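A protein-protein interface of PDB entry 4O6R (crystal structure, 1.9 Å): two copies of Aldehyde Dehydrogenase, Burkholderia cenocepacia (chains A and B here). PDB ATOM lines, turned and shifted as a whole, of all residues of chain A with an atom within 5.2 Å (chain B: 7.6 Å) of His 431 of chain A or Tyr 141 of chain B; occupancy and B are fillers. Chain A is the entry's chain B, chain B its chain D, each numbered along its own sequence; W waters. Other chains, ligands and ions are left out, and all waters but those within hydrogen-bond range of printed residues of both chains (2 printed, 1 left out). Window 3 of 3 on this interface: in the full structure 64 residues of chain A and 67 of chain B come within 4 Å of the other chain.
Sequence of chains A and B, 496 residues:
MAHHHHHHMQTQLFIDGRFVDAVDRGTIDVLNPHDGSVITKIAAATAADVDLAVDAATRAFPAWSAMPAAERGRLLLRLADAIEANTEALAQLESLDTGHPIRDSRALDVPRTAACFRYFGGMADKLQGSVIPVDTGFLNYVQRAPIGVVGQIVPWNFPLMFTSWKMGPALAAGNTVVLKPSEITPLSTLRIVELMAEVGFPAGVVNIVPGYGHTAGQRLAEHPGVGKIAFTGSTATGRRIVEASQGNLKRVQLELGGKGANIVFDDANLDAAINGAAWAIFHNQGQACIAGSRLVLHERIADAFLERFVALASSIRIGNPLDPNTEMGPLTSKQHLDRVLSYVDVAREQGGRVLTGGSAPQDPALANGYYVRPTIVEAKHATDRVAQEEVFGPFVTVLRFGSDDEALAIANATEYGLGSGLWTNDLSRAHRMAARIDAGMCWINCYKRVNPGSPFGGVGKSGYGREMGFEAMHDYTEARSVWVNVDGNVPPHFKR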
ATOM      1  N   LEU A 427      16.139  -9.021   5.948  1.00  0.00           N
ATOM      2  CA  LEU A 427      14.991  -8.311   6.472  1.00  0.00           C
ATOM      3  C   LEU A 427      14.468  -7.238   5.501  1.00  0.00           C
ATOM      4  O   LEU A 427      13.297  -7.255   5.146  1.00  0.00           O
ATOM      5  CB  LEU A 427      15.360  -7.663   7.810  1.00  0.00           C
ATOM      6  CG  LEU A 427      14.307  -6.750   8.444  1.00  0.00           C
ATOM      7  CD1 LEU A 427      13.020  -7.496   8.772  1.00  0.00           C
ATOM      8  CD2 LEU A 427      14.891  -6.137   9.678  1.00  0.00           C
ATOM      9  N   SER A 428      15.334  -6.326   5.090  1.00  0.00           N
ATOM     10  CA  SER A 428      14.922  -5.195   4.256  1.00  0.00           C
ATOM     11  C   SER A 428      14.422  -5.665   2.902  1.00  0.00           C
ATOM     12  O   SER A 428      13.384  -5.213   2.442  1.00  0.00           O
ATOM     13  CB  SER A 428      16.066  -4.189   4.074  1.00  0.00           C
ATOM     14  OG  SER A 428      16.477  -3.721   5.344  1.00  0.00           O
ATOM     15  N   ARG A 429      15.140  -6.591   2.287  1.00  0.00           N
ATOM     16  CA  ARG A 429      14.751  -7.092   0.975  1.00  0.00           C
ATOM     17  C   ARG A 429      13.345  -7.681   1.009  1.00  0.00           C
ATOM     18  O   ARG A 429      12.535  -7.421   0.098  1.00  0.00           O
ATOM     19  CB  ARG A 429      15.734  -8.136   0.473  1.00  0.00           C
ATOM     20  CG  ARG A 429      15.252  -8.885  -0.770  1.00  0.00           C
ATOM     21  CD  ARG A 429      16.206 -10.010  -1.116  1.00  0.00           C
ATOM     22  NE  ARG A 429      17.488  -9.568  -1.649  1.00  0.00           N
ATOM     23  CZ  ARG A 429      18.644 -10.200  -1.472  1.00  0.00           C
ATOM     24  NH1 ARG A 429      18.766 -11.254  -0.669  1.00  0.00           N
ATOM     25  NH2 ARG A 429      19.722  -9.741  -2.065  1.00  0.00           N
ATOM     26  N   ALA A 430      13.060  -8.460   2.053  1.00  0.00           N
ATOM     27  CA  ALA A 430      11.757  -9.141   2.151  1.00  0.00           C
ATOM     28  C   ALA A 430      10.588  -8.155   2.086  1.00  0.00           C
ATOM     29  O   ALA A 430       9.645  -8.342   1.279  1.00  0.00           O
ATOM     30  CB  ALA A 430      11.690  -9.980   3.412  1.00  0.00           C
ATOM     31  N   HIS A 431      10.663  -7.098   2.898  1.00  0.00           N
ATOM     32  CA  HIS A 431       9.592  -6.134   2.953  1.00  0.00           C
ATOM     33  C   HIS A 431       9.561  -5.237   1.719  1.00  0.00           C
ATOM     34  O   HIS A 431       8.490  -4.924   1.206  1.00  0.00           O
ATOM     35  CB  HIS A 431       9.639  -5.338   4.255  1.00  0.00           C
ATOM     36  CG  HIS A 431       9.416  -6.195   5.445  1.00  0.00           C
ATOM     37  ND1 HIS A 431       8.205  -6.799   5.698  1.00  0.00           N
ATOM     38  CD2 HIS A 431      10.274  -6.652   6.383  1.00  0.00           C
ATOM     39  CE1 HIS A 431       8.310  -7.545   6.783  1.00  0.00           C
ATOM     40  NE2 HIS A 431       9.560  -7.481   7.206  1.00  0.00           N
ATOM     41  N   ARG A 432      10.737  -4.882   1.211  1.00  0.00           N
ATOM     42  CA  ARG A 432      10.824  -3.986   0.070  1.00  0.00           C
ATOM     43  C   ARG A 432      10.278  -4.699  -1.179  1.00  0.00           C
ATOM     44  O   ARG A 432       9.459  -4.144  -1.895  1.00  0.00           O
ATOM     45  CB  ARG A 432      12.277  -3.562  -0.120  1.00  0.00           C
ATOM     46  CG  ARG A 432      12.533  -2.593  -1.245  1.00  0.00           C
ATOM     47  CD  ARG A 432      14.036  -2.518  -1.528  1.00  0.00           C
ATOM     48  NE  ARG A 432      14.793  -2.070  -0.368  1.00  0.00           N
ATOM     49  CZ  ARG A 432      15.811  -2.728   0.189  1.00  0.00           C
ATOM     50  NH1 ARG A 432      16.233  -3.919  -0.271  1.00  0.00           N
ATOM     51  NH2 ARG A 432      16.412  -2.192   1.243  1.00  0.00           N
ATOM     52  N   MET A 433      10.727  -5.933  -1.419  1.00  0.00           N
ATOM     53  CA  MET A 433      10.232  -6.690  -2.581  1.00  0.00           C
ATOM     54  C   MET A 433       8.724  -6.913  -2.471  1.00  0.00           C
ATOM     55  O   MET A 433       7.994  -6.741  -3.449  1.00  0.00           O
ATOM     56  CB  MET A 433      10.919  -8.045  -2.694  1.00  0.00           C
ATOM     57  CG  MET A 433      12.382  -7.946  -3.103  1.00  0.00           C
ATOM     58  SD  MET A 433      12.645  -7.488  -4.824  1.00  0.00           S
ATOM     59  CE  MET A 433      11.768  -8.806  -5.646  1.00  0.00           C
ATOM     60  N   ALA A 434       8.263  -7.279  -1.280  1.00  0.00           N
ATOM     61  CA  ALA A 434       6.818  -7.519  -1.087  1.00  0.00           C
ATOM     62  C   ALA A 434       5.957  -6.296  -1.457  1.00  0.00           C
ATOM     63  O   ALA A 434       4.883  -6.450  -2.056  1.00  0.00           O
ATOM     64  CB  ALA A 434       6.538  -7.965   0.333  1.00  0.00           C
ATOM     65  N   ALA A 435       6.423  -5.105  -1.115  1.00  0.00           N
ATOM     66  CA  ALA A 435       5.713  -3.874  -1.441  1.00  0.00           C
ATOM     67  C   ALA A 435       5.665  -3.594  -2.953  1.00  0.00           C
ATOM     68  O   ALA A 435       4.697  -3.041  -3.449  1.00  0.00           O
ATOM     69  CB  ALA A 435       6.328  -2.686  -0.711  1.00  0.00           C
ATOM     70  N   ILE A 444       6.404 -14.746   1.930  1.00  0.00           N
ATOM     71  CA  ILE A 444       7.838 -14.698   2.226  1.00  0.00           C
ATOM     72  C   ILE A 444       8.245 -15.918   3.037  1.00  0.00           C
ATOM     73  O   ILE A 444       7.752 -16.144   4.155  1.00  0.00           O
ATOM     74  CB  ILE A 444       8.230 -13.418   2.978  1.00  0.00           C
ATOM     75  CG1 ILE A 444       7.849 -12.198   2.114  1.00  0.00           C
ATOM     76  CG2 ILE A 444       9.728 -13.396   3.249  1.00  0.00           C
ATOM     77  CD1 ILE A 444       7.751 -10.897   2.868  1.00  0.00           C
ATOM     78  N   GLY B 129      -3.849  -0.114   7.578  1.00  0.00           N
ATOM     79  CA  GLY B 129      -3.942  -1.527   7.209  1.00  0.00           C
ATOM     80  C   GLY B 129      -4.269  -2.403   8.397  1.00  0.00           C
ATOM     81  O   GLY B 129      -4.704  -1.906   9.457  1.00  0.00           O
ATOM     82  N   SER B 130      -4.088  -3.704   8.232  1.00  0.00           N
ATOM     83  CA  SER B 130      -4.480  -4.647   9.265  1.00  0.00           C
ATOM     84  C   SER B 130      -3.470  -5.754   9.486  1.00  0.00           C
ATOM     85  O   SER B 130      -2.546  -5.940   8.683  1.00  0.00           O
ATOM     86  CB  SER B 130      -5.873  -5.180   8.986  1.00  0.00           C
ATOM     87  OG  SER B 130      -5.892  -5.798   7.717  1.00  0.00           O
ATOM     88  N   VAL B 131      -3.581  -6.421  10.627  1.00  0.00           N
ATOM     89  CA  VAL B 131      -2.741  -7.572  10.939  1.00  0.00           C
ATOM     90  C   VAL B 131      -3.712  -8.701  11.270  1.00  0.00           C
ATOM     91  O   VAL B 131      -4.571  -8.582  12.143  1.00  0.00           O
ATOM     92  CB  VAL B 131      -1.780  -7.349  12.110  1.00  0.00           C
ATOM     93  CG1 VAL B 131      -0.975  -8.612  12.388  1.00  0.00           C
ATOM     94  CG2 VAL B 131      -0.818  -6.172  11.840  1.00  0.00           C
ATOM     95  N   ILE B 132      -3.588  -9.782  10.536  1.00  0.00           N
ATOM     96  CA  ILE B 132      -4.562 -10.868  10.570  1.00  0.00           C
ATOM     97  C   ILE B 132      -4.034 -11.980  11.466  1.00  0.00           C
ATOM     98  O   ILE B 132      -2.874 -12.401  11.329  1.00  0.00           O
ATOM     99  CB  ILE B 132      -4.770 -11.486   9.172  1.00  0.00           C
ATOM    100  CG1 ILE B 132      -4.974 -10.418   8.103  1.00  0.00           C
ATOM    101  CG2 ILE B 132      -5.926 -12.482   9.182  1.00  0.00           C
ATOM    102  CD1 ILE B 132      -6.165  -9.517   8.317  1.00  0.00           C
ATOM    103  N   VAL B 134      -3.326 -15.468  12.243  1.00  0.00           N
ATOM    104  CA  VAL B 134      -3.213 -16.640  11.393  1.00  0.00           C
ATOM    105  C   VAL B 134      -2.445 -17.739  12.167  1.00  0.00           C
ATOM    106  O   VAL B 134      -2.385 -17.735  13.424  1.00  0.00           O
ATOM    107  CB  VAL B 134      -2.552 -16.273  10.037  1.00  0.00           C
ATOM    108  CG1 VAL B 134      -3.441 -15.331   9.226  1.00  0.00           C
ATOM    109  CG2 VAL B 134      -1.177 -15.656  10.263  1.00  0.00           C
ATOM    110  N   PHE B 138       3.550 -17.320  11.837  1.00  0.00           N
ATOM    111  CA  PHE B 138       3.348 -16.496  10.668  1.00  0.00           C
ATOM    112  C   PHE B 138       2.884 -15.100  11.047  1.00  0.00           C
ATOM    113  O   PHE B 138       2.015 -14.922  11.923  1.00  0.00           O
ATOM    114  CB  PHE B 138       2.290 -17.120   9.766  1.00  0.00           C
ATOM    115  CG  PHE B 138       2.742 -18.353   9.077  1.00  0.00           C
ATOM    116  CD1 PHE B 138       3.298 -18.290   7.818  1.00  0.00           C
ATOM    117  CD2 PHE B 138       2.518 -19.586   9.643  1.00  0.00           C
ATOM    118  CE1 PHE B 138       3.694 -19.448   7.152  1.00  0.00           C
ATOM    119  CE2 PHE B 138       2.901 -20.739   8.988  1.00  0.00           C
ATOM    120  CZ  PHE B 138       3.477 -20.671   7.741  1.00  0.00           C
ATOM    121  N   LEU B 139       3.430 -14.106  10.356  1.00  0.00           N
ATOM    122  CA  LEU B 139       2.956 -12.737  10.424  1.00  0.00           C
ATOM    123  C   LEU B 139       2.260 -12.410   9.118  1.00  0.00           C
ATOM    124  O   LEU B 139       2.871 -12.563   8.052  1.00  0.00           O
ATOM    125  CB  LEU B 139       4.140 -11.771  10.615  1.00  0.00           C
ATOM    126  CG  LEU B 139       3.904 -10.270  10.527  1.00  0.00           C
ATOM    127  CD1 LEU B 139       2.969  -9.861  11.653  1.00  0.00           C
ATOM    128  CD2 LEU B 139       5.220  -9.483  10.556  1.00  0.00           C
ATOM    129  N   ASN B 140       1.036 -11.873   9.193  1.00  0.00           N
ATOM    130  CA  ASN B 140       0.273 -11.505   7.993  1.00  0.00           C
ATOM    131  C   ASN B 140      -0.240 -10.100   8.163  1.00  0.00           C
ATOM    132  O   ASN B 140      -1.165  -9.855   8.997  1.00  0.00           O
ATOM    133  CB  ASN B 140      -0.873 -12.517   7.776  1.00  0.00           C
ATOM    134  CG  ASN B 140      -1.732 -12.242   6.538  1.00  0.00           C
ATOM    135  OD1 ASN B 140      -2.917 -12.664   6.488  1.00  0.00           O
ATOM    136  ND2 ASN B 140      -1.151 -11.627   5.519  1.00  0.00           N
ATOM    137  N   TYR B 141       0.396  -9.160   7.448  1.00  0.00           N
ATOM    138  CA  TYR B 141      -0.037  -7.791   7.444  1.00  0.00           C
ATOM    139  C   TYR B 141      -0.626  -7.440   6.086  1.00  0.00           C
ATOM    140  O   TYR B 141      -0.166  -7.937   5.044  1.00  0.00           O
ATOM    141  CB  TYR B 141       1.100  -6.813   7.862  1.00  0.00           C
ATOM    142  CG  TYR B 141       2.320  -6.730   6.983  1.00  0.00           C
ATOM    143  CD1 TYR B 141       3.421  -7.546   7.178  1.00  0.00           C
ATOM    144  CD2 TYR B 141       2.411  -5.746   6.002  1.00  0.00           C
ATOM    145  CE1 TYR B 141       4.552  -7.437   6.375  1.00  0.00           C
ATOM    146  CE2 TYR B 141       3.543  -5.600   5.235  1.00  0.00           C
ATOM    147  CZ  TYR B 141       4.606  -6.431   5.417  1.00  0.00           C
ATOM    148  OH  TYR B 141       5.688  -6.245   4.603  1.00  0.00           O
ATOM    149  N   VAL B 142      -1.637  -6.575   6.115  1.00  0.00           N
ATOM    150  CA  VAL B 142      -2.376  -6.157   4.926  1.00  0.00           C
ATOM    151  C   VAL B 142      -2.335  -4.634   4.829  1.00  0.00           C
ATOM    152  O   VAL B 142      -2.666  -3.925   5.777  1.00  0.00           O
ATOM    153  CB  VAL B 142      -3.828  -6.653   4.985  1.00  0.00           C
ATOM    154  CG1 VAL B 142      -4.625  -6.206   3.755  1.00  0.00           C
ATOM    155  CG2 VAL B 142      -3.864  -8.178   5.142  1.00  0.00           C
ATOM    156  N   GLN B 143      -1.866  -4.148   3.703  1.00  0.00           N
ATOM    157  CA  GLN B 143      -1.839  -2.720   3.436  1.00  0.00           C
ATOM    158  C   GLN B 143      -3.008  -2.349   2.590  1.00  0.00           C
ATOM    159  O   GLN B 143      -3.475  -3.165   1.787  1.00  0.00           O
ATOM    160  CB  GLN B 143      -0.586  -2.366   2.659  1.00  0.00           C
ATOM    161  CG  GLN B 143       0.729  -2.720   3.346  1.00  0.00           C
ATOM    162  CD  GLN B 143       1.324  -1.564   4.089  1.00  0.00           C
ATOM    163  OE1 GLN B 143       0.609  -0.686   4.606  1.00  0.00           O
ATOM    164  NE2 GLN B 143       2.642  -1.538   4.153  1.00  0.00           N
ATOM    165  N   ALA B 479      -6.355  -4.240  -1.256  1.00  0.00           N
ATOM    166  CA  ALA B 479      -5.683  -4.984  -0.194  1.00  0.00           C
ATOM    167  C   ALA B 479      -4.395  -5.571  -0.751  1.00  0.00           C
ATOM    168  O   ALA B 479      -4.412  -6.238  -1.799  1.00  0.00           O
ATOM    169  CB  ALA B 479      -6.567  -6.084   0.343  1.00  0.00           C
ATOM    170  N   ARG B 480      -3.295  -5.349  -0.038  1.00  0.00           N
ATOM    171  CA  ARG B 480      -2.016  -5.988  -0.345  1.00  0.00           C
ATOM    172  C   ARG B 480      -1.631  -6.840   0.860  1.00  0.00           C
ATOM    173  O   ARG B 480      -1.189  -6.324   1.875  1.00  0.00           O
ATOM    174  CB  ARG B 480      -0.939  -4.942  -0.643  1.00  0.00           C
ATOM    175  CG  ARG B 480      -1.126  -4.112  -1.909  1.00  0.00           C
ATOM    176  CD  ARG B 480      -1.220  -4.979  -3.122  1.00  0.00           C
ATOM    177  NE  ARG B 480      -0.855  -4.330  -4.385  1.00  0.00           N
ATOM    178  CZ  ARG B 480       0.366  -4.335  -4.923  1.00  0.00           C
ATOM    179  NH1 ARG B 480       1.416  -4.858  -4.298  1.00  0.00           N
ATOM    180  NH2 ARG B 480       0.547  -3.767  -6.093  1.00  0.00           N
ATOM    181  N   SER B 481      -1.824  -8.142   0.763  1.00  0.00           N
ATOM    182  CA  SER B 481      -1.575  -9.053   1.890  1.00  0.00           C
ATOM    183  C   SER B 481      -0.138  -9.638   1.798  1.00  0.00           C
ATOM    184  O   SER B 481       0.245 -10.199   0.755  1.00  0.00           O
ATOM    185  CB  SER B 481      -2.593 -10.189   1.827  1.00  0.00           C
ATOM    186  OG  SER B 481      -2.304 -11.173   2.778  1.00  0.00           O
ATOM    187  N   VAL B 482       0.640  -9.476   2.856  1.00  0.00           N
ATOM    188  CA  VAL B 482       2.005 -10.001   2.936  1.00  0.00           C
ATOM    189  C   VAL B 482       2.092 -10.973   4.092  1.00  0.00           C
ATOM    190  O   VAL B 482       1.639 -10.685   5.215  1.00  0.00           O
ATOM    191  CB  VAL B 482       3.019  -8.845   3.139  1.00  0.00           C
ATOM    192  CG1 VAL B 482       4.440  -9.348   3.218  1.00  0.00           C
ATOM    193  CG2 VAL B 482       2.839  -7.783   2.034  1.00  0.00           C
ATOM    194  N   TRP B 483       2.717 -12.122   3.827  1.00  0.00           N
ATOM    195  CA  TRP B 483       2.916 -13.146   4.822  1.00  0.00           C
ATOM    196  C   TRP B 483       4.404 -13.315   5.072  1.00  0.00           C
ATOM    197  O   TRP B 483       5.167 -13.410   4.138  1.00  0.00           O
ATOM    198  CB  TRP B 483       2.400 -14.486   4.355  1.00  0.00           C
ATOM    199  CG  TRP B 483       0.924 -14.590   4.211  1.00  0.00           C
ATOM    200  CD1 TRP B 483       0.138 -14.010   3.248  1.00  0.00           C
ATOM    201  CD2 TRP B 483       0.066 -15.404   5.002  1.00  0.00           C
ATOM    202  NE1 TRP B 483      -1.158 -14.395   3.428  1.00  0.00           N
ATOM    203  CE2 TRP B 483      -1.234 -15.260   4.488  1.00  0.00           C
ATOM    204  CE3 TRP B 483       0.274 -16.225   6.112  1.00  0.00           C
ATOM    205  CZ2 TRP B 483      -2.328 -15.924   5.026  1.00  0.00           C
ATOM    206  CZ3 TRP B 483      -0.816 -16.910   6.653  1.00  0.00           C
ATOM    207  CH2 TRP B 483      -2.105 -16.749   6.103  1.00  0.00           C
ATOM    208  N   VAL B 484       4.793 -13.349   6.337  1.00  0.00           N
ATOM    209  CA  VAL B 484       6.159 -13.711   6.682  1.00  0.00           C
ATOM    210  C   VAL B 484       6.124 -14.984   7.491  1.00  0.00           C
ATOM    211  O   VAL B 484       5.532 -15.024   8.584  1.00  0.00           O
ATOM    212  CB  VAL B 484       6.911 -12.631   7.467  1.00  0.00           C
ATOM    213  CG1 VAL B 484       8.379 -13.010   7.609  1.00  0.00           C
ATOM    214  CG2 VAL B 484       6.778 -11.277   6.773  1.00  0.00           C
HETATM  215  O   HOH W   1       2.304  -5.715  -1.645  1.00  0.00           O
HETATM  216  O   HOH W   2       6.100  -4.432   2.696  1.00  0.00           O
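ND1 of His 431 of chain A sits at hydrogen-bond distance from OH of Tyr 141 of chain B.
O of Trp 483 of chain B lies within hydrogen-bond range of N of Ile 444 of chain A.
The backbone carbonyl oxygen of Leu 139 of chain B lies within hydrogen-bond range of the backbone NH of Val 484 of chain B (2.7 Å).
The backbone carbonyl oxygen of Val 482 of chain B is in hydrogen-bond range of the side-chain amide nitrogen of Asn 140 of chain B, 3.0 Å away.
The indole nitrogen (NE1) of Trp 483 of chain B sits close to the side-chain amide nitrogen (ND2) of Asn 140 of chain B (3.5 Å).
The backbone carbonyl oxygen of Tyr 141 of chain B sits at hydrogen-bond distance from the backbone NH of Val 482 of chain B (2.8 Å).
O of Gln 143 of chain B lies within hydrogen-bond range of N of Arg 480 of chain B (2.9 Å).
The side-chain hydroxyl of Ser 481 of chain B sits at hydrogen-bond distance from the indole nitrogen of Trp 483 of chain B (3.5 Å).
Among the printed residues, pairs that only touch across the chains: Ile 444 of chain A with Val 482 of chain B (3.7 Å), Ala 434 of chain A with Val 482 of chain B (3.8 Å), Ala 435 of chain A with Arg 480 of chain B (3.8 Å) and Ile 444 of chain A with Val 484 of chain B (3.9 Å).
Arg 429 of chain A touches none of the printed residues of chain B.
Of the printed residues of chain B, His 431 of chain A touches Tyr 141.
Printed residues of chain B within 4 Å of Ala 435 of chain A: Arg 480.
Of the printed residues of chain B, Ile 444 of chain A touches Val 482 (3.7 Å), Trp 483 (2.9 Å) and Val 484 (3.9 Å).
Ile 132 of chain B touches none of the printed residues of chain A.
Tyr 141 of chain B touches one residue of chain A.
Of the printed residues of chain A, Val 482 of chain B touches Ala 434 and Ile 444.
Printed residues of chain A within 4 Å of Trp 483 of chain B: Ile 444.
Printed residues of chain A within 4 Å of Val 484 of chain B: Ile 444.
The nearest residue of chain B that does not touch His 431 of chain A is Val 484 of chain B (4.03 Å).
The nearest residue of chain A that does not touch Tyr 141 of chain B is Ala 434 of chain A (4.7 Å).
Hydrophobic or aromatic side chains of chain B within 4 Å of the printed part of chain A: Tyr 141 and Val 482.
Along chain B the printed residues that touch a printed residue of chain A span positions 141 to 484.
Hydrophobic or aromatic side chains of chain A that line the printed part of chain B: His 431, Ala 434 and Ile 444.
No position is printed for both chains.
Of the 6 pairs that touch across the chains among the printed residues, none has its exchanged pair printed and touching as well.
Water W2 bridges OH of Tyr 141 of chain B and O of His 431 of chain A.
Water W1 lies within hydrogen-bond range of O of Ala 434 of chain A (2.7 Å) and NH1 of Arg 480 of chain B (2.9 Å).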
